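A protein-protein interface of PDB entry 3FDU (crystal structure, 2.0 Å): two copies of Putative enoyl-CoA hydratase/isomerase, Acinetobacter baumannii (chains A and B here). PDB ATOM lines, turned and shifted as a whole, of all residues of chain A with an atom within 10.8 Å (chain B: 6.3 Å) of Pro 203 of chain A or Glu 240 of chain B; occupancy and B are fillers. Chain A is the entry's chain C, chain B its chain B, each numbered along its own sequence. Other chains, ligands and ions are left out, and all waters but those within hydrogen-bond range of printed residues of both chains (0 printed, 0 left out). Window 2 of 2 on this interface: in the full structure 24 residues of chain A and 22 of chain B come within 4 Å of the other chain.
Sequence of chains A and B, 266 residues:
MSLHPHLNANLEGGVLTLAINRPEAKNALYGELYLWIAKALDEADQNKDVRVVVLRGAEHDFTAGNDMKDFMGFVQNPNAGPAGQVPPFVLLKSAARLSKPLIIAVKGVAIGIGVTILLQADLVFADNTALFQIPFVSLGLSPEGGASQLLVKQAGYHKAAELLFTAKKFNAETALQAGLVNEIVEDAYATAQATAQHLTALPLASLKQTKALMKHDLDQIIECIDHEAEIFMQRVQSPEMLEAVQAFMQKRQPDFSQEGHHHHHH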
ATOM      1  N   VAL A  50      16.955  19.334  24.051  1.00  0.00           N
ATOM      2  CA  VAL A  50      16.891  20.599  24.822  1.00  0.00           C
ATOM      3  C   VAL A  50      17.976  21.580  24.375  1.00  0.00           C
ATOM      4  O   VAL A  50      19.165  21.264  24.407  1.00  0.00           O
ATOM      5  CB  VAL A  50      17.014  20.340  26.331  1.00  0.00           C
ATOM      6  CG1 VAL A  50      16.811  21.649  27.123  1.00  0.00           C
ATOM      7  CG2 VAL A  50      16.011  19.272  26.762  1.00  0.00           C
ATOM      8  N   ARG A  51      17.555  22.766  23.966  1.00  0.00           N
ATOM      9  CA  ARG A  51      18.479  23.824  23.593  1.00  0.00           C
ATOM     10  C   ARG A  51      18.479  24.996  24.610  1.00  0.00           C
ATOM     11  O   ARG A  51      19.504  25.644  24.810  1.00  0.00           O
ATOM     12  CB  ARG A  51      18.116  24.352  22.200  1.00  0.00           C
ATOM     13  CG  ARG A  51      18.259  23.279  21.073  1.00  0.00           C
ATOM     14  CD  ARG A  51      17.642  23.794  19.747  1.00  0.00           C
ATOM     15  NE  ARG A  51      18.637  24.623  19.081  1.00  0.00           N
ATOM     16  CZ  ARG A  51      18.875  24.647  17.770  1.00  0.00           C
ATOM     17  NH1 ARG A  51      18.149  23.892  16.934  1.00  0.00           N
ATOM     18  NH2 ARG A  51      19.839  25.440  17.288  1.00  0.00           N
ATOM     19  N   VAL A  52      17.326  25.272  25.216  1.00  0.00           N
ATOM     20  CA  VAL A  52      17.219  26.350  26.222  1.00  0.00           C
ATOM     21  C   VAL A  52      16.328  25.886  27.349  1.00  0.00           C
ATOM     22  O   VAL A  52      15.385  25.131  27.103  1.00  0.00           O
ATOM     23  CB  VAL A  52      16.641  27.644  25.628  1.00  0.00           C
ATOM     24  CG1 VAL A  52      16.603  28.792  26.700  1.00  0.00           C
ATOM     25  CG2 VAL A  52      17.410  28.065  24.377  1.00  0.00           C
ATOM     26  N   SER A  99      25.058  24.150  30.740  1.00  0.00           N
ATOM     27  CA  SER A  99      25.880  24.708  29.664  1.00  0.00           C
ATOM     28  C   SER A  99      25.044  25.458  28.659  1.00  0.00           C
ATOM     29  O   SER A  99      25.566  26.250  27.901  1.00  0.00           O
ATOM     30  CB  SER A  99      26.697  23.610  28.942  1.00  0.00           C
ATOM     31  OG  SER A  99      25.876  22.883  28.041  1.00  0.00           O
ATOM     32  N   LYS A 100      23.738  25.209  28.657  1.00  0.00           N
ATOM     33  CA  LYS A 100      22.828  25.887  27.774  1.00  0.00           C
ATOM     34  C   LYS A 100      22.168  27.094  28.474  1.00  0.00           C
ATOM     35  O   LYS A 100      22.211  27.230  29.696  1.00  0.00           O
ATOM     36  CB  LYS A 100      21.762  24.881  27.289  1.00  0.00           C
ATOM     37  CG  LYS A 100      22.366  23.607  26.636  1.00  0.00           C
ATOM     38  CD  LYS A 100      21.424  22.387  26.731  1.00  0.00           C
ATOM     39  CE  LYS A 100      21.997  21.163  25.989  1.00  0.00           C
ATOM     40  NZ  LYS A 100      20.941  20.109  25.892  1.00  0.00           N
ATOM     41  N   PRO A 101      21.536  27.971  27.698  1.00  0.00           N
ATOM     42  CA  PRO A 101      21.013  29.162  28.375  1.00  0.00           C
ATOM     43  C   PRO A 101      19.938  28.806  29.390  1.00  0.00           C
ATOM     44  O   PRO A 101      19.070  27.950  29.127  1.00  0.00           O
ATOM     45  CB  PRO A 101      20.402  29.988  27.239  1.00  0.00           C
ATOM     46  CG  PRO A 101      21.126  29.449  25.941  1.00  0.00           C
ATOM     47  CD  PRO A 101      21.294  27.982  26.239  1.00  0.00           C
ATOM     48  N   ALA A 196      13.143  32.608  24.851  1.00  0.00           N
ATOM     49  CA  ALA A 196      13.680  31.266  24.699  1.00  0.00           C
ATOM     50  C   ALA A 196      13.520  30.754  23.257  1.00  0.00           C
ATOM     51  O   ALA A 196      14.325  29.946  22.784  1.00  0.00           O
ATOM     52  CB  ALA A 196      13.039  30.273  25.703  1.00  0.00           C
ATOM     53  N   GLN A 197      12.480  31.227  22.582  1.00  0.00           N
ATOM     54  CA  GLN A 197      12.187  30.775  21.212  1.00  0.00           C
ATOM     55  C   GLN A 197      13.142  31.430  20.247  1.00  0.00           C
ATOM     56  O   GLN A 197      13.554  30.833  19.249  1.00  0.00           O
ATOM     57  CB  GLN A 197      10.768  31.182  20.826  1.00  0.00           C
ATOM     58  CG  GLN A 197       9.724  30.262  21.341  1.00  0.00           C
ATOM     59  CD  GLN A 197       8.327  30.808  21.117  1.00  0.00           C
ATOM     60  OE1 GLN A 197       7.356  30.056  21.045  1.00  0.00           O
ATOM     61  NE2 GLN A 197       8.220  32.123  21.009  1.00  0.00           N
ATOM     62  N   HIS A 198      13.473  32.679  20.528  1.00  0.00           N
ATOM     63  CA  HIS A 198      14.512  33.371  19.766  1.00  0.00           C
ATOM     64  C   HIS A 198      15.844  32.657  19.905  1.00  0.00           C
ATOM     65  O   HIS A 198      16.546  32.458  18.895  1.00  0.00           O
ATOM     66  CB  HIS A 198      14.652  34.827  20.214  1.00  0.00           C
ATOM     67  CG  HIS A 198      15.801  35.545  19.561  1.00  0.00           C
ATOM     68  ND1 HIS A 198      15.884  35.736  18.195  1.00  0.00           N
ATOM     69  CD2 HIS A 198      16.924  36.102  20.086  1.00  0.00           C
ATOM     70  CE1 HIS A 198      16.999  36.394  17.909  1.00  0.00           C
ATOM     71  NE2 HIS A 198      17.647  36.626  19.039  1.00  0.00           N
ATOM     72  N   LEU A 199      16.209  32.280  21.136  1.00  0.00           N
ATOM     73  CA  LEU A 199      17.466  31.577  21.365  1.00  0.00           C
ATOM     74  C   LEU A 199      17.520  30.142  20.779  1.00  0.00           C
ATOM     75  O   LEU A 199      18.581  29.729  20.311  1.00  0.00           O
ATOM     76  CB  LEU A 199      17.875  31.564  22.835  1.00  0.00           C
ATOM     77  CG  LEU A 199      18.047  32.888  23.631  1.00  0.00           C
ATOM     78  CD1 LEU A 199      18.521  32.548  25.081  1.00  0.00           C
ATOM     79  CD2 LEU A 199      19.000  33.844  22.917  1.00  0.00           C
ATOM     80  N   THR A 200      16.416  29.385  20.808  1.00  0.00           N
ATOM     81  CA  THR A 200      16.420  28.055  20.148  1.00  0.00           C
ATOM     82  C   THR A 200      16.610  28.153  18.641  1.00  0.00           C
ATOM     83  O   THR A 200      17.102  27.215  18.055  1.00  0.00           O
ATOM     84  CB  THR A 200      15.119  27.241  20.339  1.00  0.00           C
ATOM     85  OG1 THR A 200      14.041  27.959  19.727  1.00  0.00           O
ATOM     86  CG2 THR A 200      14.818  27.034  21.786  1.00  0.00           C
ATOM     87  N   ALA A 201      16.224  29.267  18.016  1.00  0.00           N
ATOM     88  CA  ALA A 201      16.454  29.455  16.560  1.00  0.00           C
ATOM     89  C   ALA A 201      17.909  29.775  16.213  1.00  0.00           C
ATOM     90  O   ALA A 201      18.272  29.794  15.035  1.00  0.00           O
ATOM     91  CB  ALA A 201      15.562  30.554  16.010  1.00  0.00           C
ATOM     92  N   LEU A 202      18.742  30.043  17.222  1.00  0.00           N
ATOM     93  CA  LEU A 202      20.108  30.443  16.965  1.00  0.00           C
ATOM     94  C   LEU A 202      21.061  29.253  17.168  1.00  0.00           C
ATOM     95  O   LEU A 202      20.711  28.241  17.798  1.00  0.00           O
ATOM     96  CB  LEU A 202      20.519  31.683  17.825  1.00  0.00           C
ATOM     97  CG  LEU A 202      19.789  33.044  17.667  1.00  0.00           C
ATOM     98  CD1 LEU A 202      20.156  34.102  18.793  1.00  0.00           C
ATOM     99  CD2 LEU A 202      19.939  33.709  16.289  1.00  0.00           C
ATOM    100  N   PRO A 203      22.277  29.372  16.639  1.00  0.00           N
ATOM    101  CA  PRO A 203      23.185  28.232  16.653  1.00  0.00           C
ATOM    102  C   PRO A 203      23.565  27.805  18.055  1.00  0.00           C
ATOM    103  O   PRO A 203      24.202  28.575  18.782  1.00  0.00           O
ATOM    104  CB  PRO A 203      24.426  28.754  15.913  1.00  0.00           C
ATOM    105  CG  PRO A 203      23.928  29.936  15.093  1.00  0.00           C
ATOM    106  CD  PRO A 203      22.835  30.542  15.947  1.00  0.00           C
ATOM    107  N   LEU A 204      23.238  26.561  18.411  1.00  0.00           N
ATOM    108  CA  LEU A 204      23.520  26.071  19.753  1.00  0.00           C
ATOM    109  C   LEU A 204      25.015  26.103  20.015  1.00  0.00           C
ATOM    110  O   LEU A 204      25.461  26.376  21.128  1.00  0.00           O
ATOM    111  CB  LEU A 204      22.975  24.655  19.955  1.00  0.00           C
ATOM    112  CG  LEU A 204      23.395  24.035  21.293  1.00  0.00           C
ATOM    113  CD1 LEU A 204      22.253  23.265  21.971  1.00  0.00           C
ATOM    114  CD2 LEU A 204      24.639  23.173  21.165  1.00  0.00           C
ATOM    115  N   ALA A 205      25.805  25.806  18.987  1.00  0.00           N
ATOM    116  CA  ALA A 205      27.238  25.804  19.139  1.00  0.00           C
ATOM    117  C   ALA A 205      27.744  27.204  19.524  1.00  0.00           C
ATOM    118  O   ALA A 205      28.667  27.336  20.326  1.00  0.00           O
ATOM    119  CB  ALA A 205      27.905  25.335  17.849  1.00  0.00           C
ATOM    120  N   SER A 206      27.161  28.245  18.937  1.00  0.00           N
ATOM    121  CA  SER A 206      27.592  29.609  19.269  1.00  0.00           C
ATOM    122  C   SER A 206      27.194  29.981  20.716  1.00  0.00           C
ATOM    123  O   SER A 206      27.994  30.542  21.461  1.00  0.00           O
ATOM    124  CB  SER A 206      27.051  30.612  18.259  1.00  0.00           C
ATOM    125  OG  SER A 206      27.794  30.529  17.047  1.00  0.00           O
ATOM    126  N   LEU A 207      25.968  29.641  21.109  1.00  0.00           N
ATOM    127  CA  LEU A 207      25.498  29.950  22.463  1.00  0.00           C
ATOM    128  C   LEU A 207      26.326  29.215  23.492  1.00  0.00           C
ATOM    129  O   LEU A 207      26.787  29.808  24.474  1.00  0.00           O
ATOM    130  CB  LEU A 207      24.027  29.600  22.619  1.00  0.00           C
ATOM    131  CG  LEU A 207      23.161  30.544  21.830  1.00  0.00           C
ATOM    132  CD1 LEU A 207      21.746  29.955  21.718  1.00  0.00           C
ATOM    133  CD2 LEU A 207      23.164  31.940  22.479  1.00  0.00           C
ATOM    134  N   LYS A 208      26.575  27.937  23.234  1.00  0.00           N
ATOM    135  CA  LYS A 208      27.349  27.103  24.153  1.00  0.00           C
ATOM    136  C   LYS A 208      28.749  27.708  24.354  1.00  0.00           C
ATOM    137  O   LYS A 208      29.224  27.918  25.485  1.00  0.00           O
ATOM    138  CB  LYS A 208      27.468  25.682  23.570  1.00  0.00           C
ATOM    139  CG  LYS A 208      27.835  24.584  24.542  1.00  0.00           C
ATOM    140  CD  LYS A 208      28.833  23.582  23.902  1.00  0.00           C
ATOM    141  CE  LYS A 208      28.868  22.190  24.573  1.00  0.00           C
ATOM    142  NZ  LYS A 208      28.784  22.258  26.036  1.00  0.00           N
ATOM    143  N   GLN A 209      29.433  27.959  23.246  1.00  0.00           N
ATOM    144  CA  GLN A 209      30.790  28.473  23.327  1.00  0.00           C
ATOM    145  C   GLN A 209      30.873  29.908  23.894  1.00  0.00           C
ATOM    146  O   GLN A 209      31.800  30.233  24.603  1.00  0.00           O
ATOM    147  CB  GLN A 209      31.471  28.396  21.949  1.00  0.00           C
ATOM    148  CG  GLN A 209      32.850  28.960  21.981  1.00  0.00           C
ATOM    149  CD  GLN A 209      33.807  28.072  22.738  1.00  0.00           C
ATOM    150  OE1 GLN A 209      34.334  27.107  22.175  1.00  0.00           O
ATOM    151  NE2 GLN A 209      34.076  28.407  24.013  1.00  0.00           N
ATOM    152  N   THR A 210      29.903  30.752  23.576  1.00  0.00           N
ATOM    153  CA  THR A 210      29.851  32.106  24.156  1.00  0.00           C
ATOM    154  C   THR A 210      29.680  32.043  25.681  1.00  0.00           C
ATOM    155  O   THR A 210      30.375  32.717  26.413  1.00  0.00           O
ATOM    156  CB  THR A 210      28.726  32.909  23.556  1.00  0.00           C
ATOM    157  OG1 THR A 210      28.991  33.124  22.166  1.00  0.00           O
ATOM    158  CG2 THR A 210      28.604  34.246  24.224  1.00  0.00           C
ATOM    159  N   LYS A 211      28.775  31.195  26.150  1.00  0.00           N
ATOM    160  CA  LYS A 211      28.531  31.060  27.598  1.00  0.00           C
ATOM    161  C   LYS A 211      29.725  30.474  28.316  1.00  0.00           C
ATOM    162  O   LYS A 211      30.078  30.894  29.428  1.00  0.00           O
ATOM    163  CB  LYS A 211      27.253  30.239  27.873  1.00  0.00           C
ATOM    164  CG  LYS A 211      26.992  30.011  29.362  1.00  0.00           C
ATOM    165  CD  LYS A 211      25.553  29.555  29.670  1.00  0.00           C
ATOM    166  CE  LYS A 211      25.329  29.333  31.174  1.00  0.00           C
ATOM    167  NZ  LYS A 211      23.897  28.862  31.400  1.00  0.00           N
ATOM    168  N   VAL B 137      26.697  35.876  17.541  1.00  0.00           N
ATOM    169  CA  VAL B 137      25.991  34.617  17.798  1.00  0.00           C
ATOM    170  C   VAL B 137      25.101  34.206  16.645  1.00  0.00           C
ATOM    171  O   VAL B 137      25.042  33.004  16.295  1.00  0.00           O
ATOM    172  CB  VAL B 137      25.140  34.602  19.083  1.00  0.00           C
ATOM    173  CG1 VAL B 137      24.056  33.466  18.976  1.00  0.00           C
ATOM    174  CG2 VAL B 137      26.015  34.360  20.288  1.00  0.00           C
ATOM    175  N   SER B 138      24.398  35.176  16.063  1.00  0.00           N
ATOM    176  CA  SER B 138      23.537  34.867  14.935  1.00  0.00           C
ATOM    177  C   SER B 138      24.272  34.657  13.592  1.00  0.00           C
ATOM    178  O   SER B 138      23.634  34.342  12.579  1.00  0.00           O
ATOM    179  CB  SER B 138      22.435  35.905  14.773  1.00  0.00           C
ATOM    180  OG  SER B 138      22.989  37.194  14.594  1.00  0.00           O
ATOM    181  N   LEU B 139      25.588  34.843  13.570  1.00  0.00           N
ATOM    182  CA  LEU B 139      26.357  34.577  12.355  1.00  0.00           C
ATOM    183  C   LEU B 139      26.988  33.222  12.479  1.00  0.00           C
ATOM    184  O   LEU B 139      27.713  32.792  11.591  1.00  0.00           O
ATOM    185  CB  LEU B 139      27.452  35.622  12.156  1.00  0.00           C
ATOM    186  CG  LEU B 139      26.864  36.992  11.883  1.00  0.00           C
ATOM    187  CD1 LEU B 139      27.971  37.983  11.766  1.00  0.00           C
ATOM    188  CD2 LEU B 139      26.035  36.918  10.606  1.00  0.00           C
ATOM    189  N   GLY B 140      26.711  32.540  13.585  1.00  0.00           N
ATOM    190  CA  GLY B 140      27.322  31.242  13.846  1.00  0.00           C
ATOM    191  C   GLY B 140      28.725  31.368  14.393  1.00  0.00           C
ATOM    192  O   GLY B 140      29.502  30.400  14.416  1.00  0.00           O
ATOM    193  N   LEU B 141      29.053  32.559  14.882  1.00  0.00           N
ATOM    194  CA  LEU B 141      30.407  32.839  15.328  1.00  0.00           C
ATOM    195  C   LEU B 141      30.494  32.858  16.856  1.00  0.00           C
ATOM    196  O   LEU B 141      29.824  32.077  17.530  1.00  0.00           O
ATOM    197  CB  LEU B 141      30.934  34.136  14.666  1.00  0.00           C
ATOM    198  CG  LEU B 141      30.882  34.027  13.132  1.00  0.00           C
ATOM    199  CD1 LEU B 141      30.952  35.367  12.373  1.00  0.00           C
ATOM    200  CD2 LEU B 141      31.979  33.083  12.649  1.00  0.00           C
ATOM    201  N   ARG B 235      35.117  28.794  14.474  1.00  0.00           N
ATOM    202  CA  ARG B 235      33.715  28.916  14.151  1.00  0.00           C
ATOM    203  C   ARG B 235      33.579  29.413  12.723  1.00  0.00           C
ATOM    204  O   ARG B 235      32.582  29.134  12.067  1.00  0.00           O
ATOM    205  CB  ARG B 235      32.993  29.871  15.114  1.00  0.00           C
ATOM    206  CG  ARG B 235      32.898  29.360  16.556  1.00  0.00           C
ATOM    207  CD  ARG B 235      31.520  28.829  16.895  1.00  0.00           C
ATOM    208  NE  ARG B 235      31.305  27.476  16.409  1.00  0.00           N
ATOM    209  CZ  ARG B 235      30.290  27.101  15.644  1.00  0.00           C
ATOM    210  NH1 ARG B 235      30.200  25.847  15.262  1.00  0.00           N
ATOM    211  NH2 ARG B 235      29.360  27.969  15.263  1.00  0.00           N
ATOM    212  N   SER B 238      32.651  26.686   9.972  1.00  0.00           N
ATOM    213  CA  SER B 238      31.585  25.821  10.482  1.00  0.00           C
ATOM    214  C   SER B 238      30.264  25.960   9.702  1.00  0.00           C
ATOM    215  O   SER B 238      29.936  27.022   9.147  1.00  0.00           O
ATOM    216  CB  SER B 238      31.340  26.080  11.985  1.00  0.00           C
ATOM    217  OG  SER B 238      30.363  27.103  12.191  1.00  0.00           O
ATOM    218  N   PRO B 239      29.493  24.872   9.652  1.00  0.00           N
ATOM    219  CA  PRO B 239      28.218  24.854   8.938  1.00  0.00           C
ATOM    220  C   PRO B 239      27.245  25.959   9.394  1.00  0.00           C
ATOM    221  O   PRO B 239      26.573  26.591   8.561  1.00  0.00           O
ATOM    222  CB  PRO B 239      27.656  23.461   9.251  1.00  0.00           C
ATOM    223  CG  PRO B 239      28.655  22.790  10.146  1.00  0.00           C
ATOM    224  CD  PRO B 239      29.930  23.533  10.059  1.00  0.00           C
ATOM    225  N   GLU B 240      27.178  26.183  10.706  1.00  0.00           N
ATOM    226  CA  GLU B 240      26.419  27.294  11.267  1.00  0.00           C
ATOM    227  C   GLU B 240      26.695  28.580  10.504  1.00  0.00           C
ATOM    228  O   GLU B 240      25.777  29.266  10.068  1.00  0.00           O
ATOM    229  CB  GLU B 240      26.806  27.504  12.734  1.00  0.00           C
ATOM    230  CG  GLU B 240      26.148  26.546  13.705  1.00  0.00           C
ATOM    231  CD  GLU B 240      26.825  25.197  13.768  1.00  0.00           C
ATOM    232  OE1 GLU B 240      28.086  25.141  13.826  1.00  0.00           O
ATOM    233  OE2 GLU B 240      26.083  24.186  13.774  1.00  0.00           O
ATOM    234  N   MET B 241      27.976  28.904  10.362  1.00  0.00           N
ATOM    235  CA  MET B 241      28.421  30.115   9.676  1.00  0.00           C
ATOM    236  C   MET B 241      27.904  30.152   8.230  1.00  0.00           C
ATOM    237  O   MET B 241      27.388  31.170   7.771  1.00  0.00           O
ATOM    238  CB  MET B 241      29.961  30.198   9.720  1.00  0.00           C
ATOM    239  CG  MET B 241      30.592  31.179   8.737  1.00  0.00           C
ATOM    240  SD  MET B 241      30.436  32.835   9.341  1.00  0.00           S
ATOM    241  CE  MET B 241      30.521  33.789   7.838  1.00  0.00           C
ATOM    242  N   LEU B 242      28.048  29.029   7.526  1.00  0.00           N
ATOM    243  CA  LEU B 242      27.622  28.931   6.126  1.00  0.00           C
ATOM    244  C   LEU B 242      26.131  29.228   5.996  1.00  0.00           C
ATOM    245  O   LEU B 242      25.736  30.119   5.246  1.00  0.00           O
ATOM    246  CB  LEU B 242      27.964  27.544   5.545  1.00  0.00           C
ATOM    247  N   GLU B 243      25.314  28.493   6.746  1.00  0.00           N
ATOM    248  CA  GLU B 243      23.869  28.740   6.773  1.00  0.00           C
ATOM    249  C   GLU B 243      23.580  30.180   7.148  1.00  0.00           C
ATOM    250  O   GLU B 243      23.036  30.929   6.347  1.00  0.00           O
ATOM    251  CB  GLU B 243      23.168  27.811   7.757  1.00  0.00           C
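The side-chain hydroxyl (OG) of Ser 206 of chain A is in hydrogen-bond range of the guanidinium group (NH2) of Arg 235 of chain B (3.5 Å). O of Gly 140 of chain B sits close to OG of Ser 206 of chain A (3.1 Å). The backbone carbonyl oxygen (O) of Leu 141 of chain B lies within hydrogen-bond range of the side-chain hydroxyl (OG) of Ser 206 of chain A (2.6 Å).
The side-chain carboxylate (OE1) of Glu 240 of chain B is in hydrogen-bond range of the side-chain hydroxyl (OG) of Ser 238 of chain B (3.4 Å). The guanidinium group of Arg 235 of chain B is in salt-bridge range of the side-chain carboxylate of Glu 240 of chain B (2.7 Å). NH2 of Arg 235 of chain B sits at hydrogen-bond distance from O of Gly 140 of chain B (2.6 Å). The backbone carbonyl oxygen (O) of Arg 235 of chain B sits at hydrogen-bond distance from the side-chain hydroxyl (OG) of Ser 238 of chain B (3.0 Å). O of Ser 206 of chain A sits at hydrogen-bond distance from OG1 of Thr 210 of chain A. NH2 of Arg 51 of chain A sits at hydrogen-bond distance from O of Leu 202 of chain A (3.0 Å).
Leu 202 of chain A touches Val 137 of chain B. Leu 202 of chain A touches Ser 138 of chain B. Val 137 of chain B touches Pro 203 of chain A (O to CD, 3.3 Å). Pro 203 of chain A touches Gly 140 of chain B (CG to CA, 3.8 Å). Pro 203 of chain A touches Glu 240 of chain B (CB to CG, 3.6 Å). CB of Ala 205 of chain A touches NH1 of Arg 235 of chain B, 3.5 Å away. Ser 206 of chain A touches Val 137 of chain B (CB to O, 3.7 Å). Leu 207 of chain A touches Val 137 of chain B (CD2 to CG1, 3.9 Å). Thr 210 of chain A touches Val 137 of chain B (OG1 to CG2, 3.7 Å).
Of the printed residues of chain B, Pro 203 of chain A touches Val 137 (3.3 Å), Gly 140 (3.8 Å) and Glu 240 (3.6 Å). Printed residues of chain A within 4 Å of Glu 240 of chain B: Pro 203. Of the printed residues of chain A, Gly 140 of chain B touches Pro 203 and Ser 206. No residue of chain A comes within 4 Å of Pro 239 of chain B. No residue of chain A comes within 4 Å of Leu 242 of chain B. No residue of chain A comes within 4 Å of Glu 243 of chain B. Of the printed residues of chain A, Leu 141 of chain B touches Ser 206 (2.6 Å). Of the printed residues of chain B, Leu 207 of chain A touches Val 137. The nearest residue of chain B that does not touch Pro 203 of chain A is Ser 138 of chain B (4.5 Å). The nearest printed residue of chain A that does not touch Leu 141 of chain B is Thr 210 of chain A (4.8 Å).
Of the 12 printed residues of chain B, 6 touch a printed residue of chain A. Of the 22 printed residues of chain A, 6 touch a printed residue of chain B. Hydrophobic or aromatic side chains of chain A within 4 Å of the printed part of chain B: Leu 202, Pro 203, Ala 205 and Leu 207. Among the printed residues, no Asp or Glu carboxylate lies within 4 Å of a Lys or Arg side-chain nitrogen of the other chain.
No position is printed for both chains. Of the 12 pairs that touch across the chains among the printed residues, none has its exchanged pair printed and touching as well.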
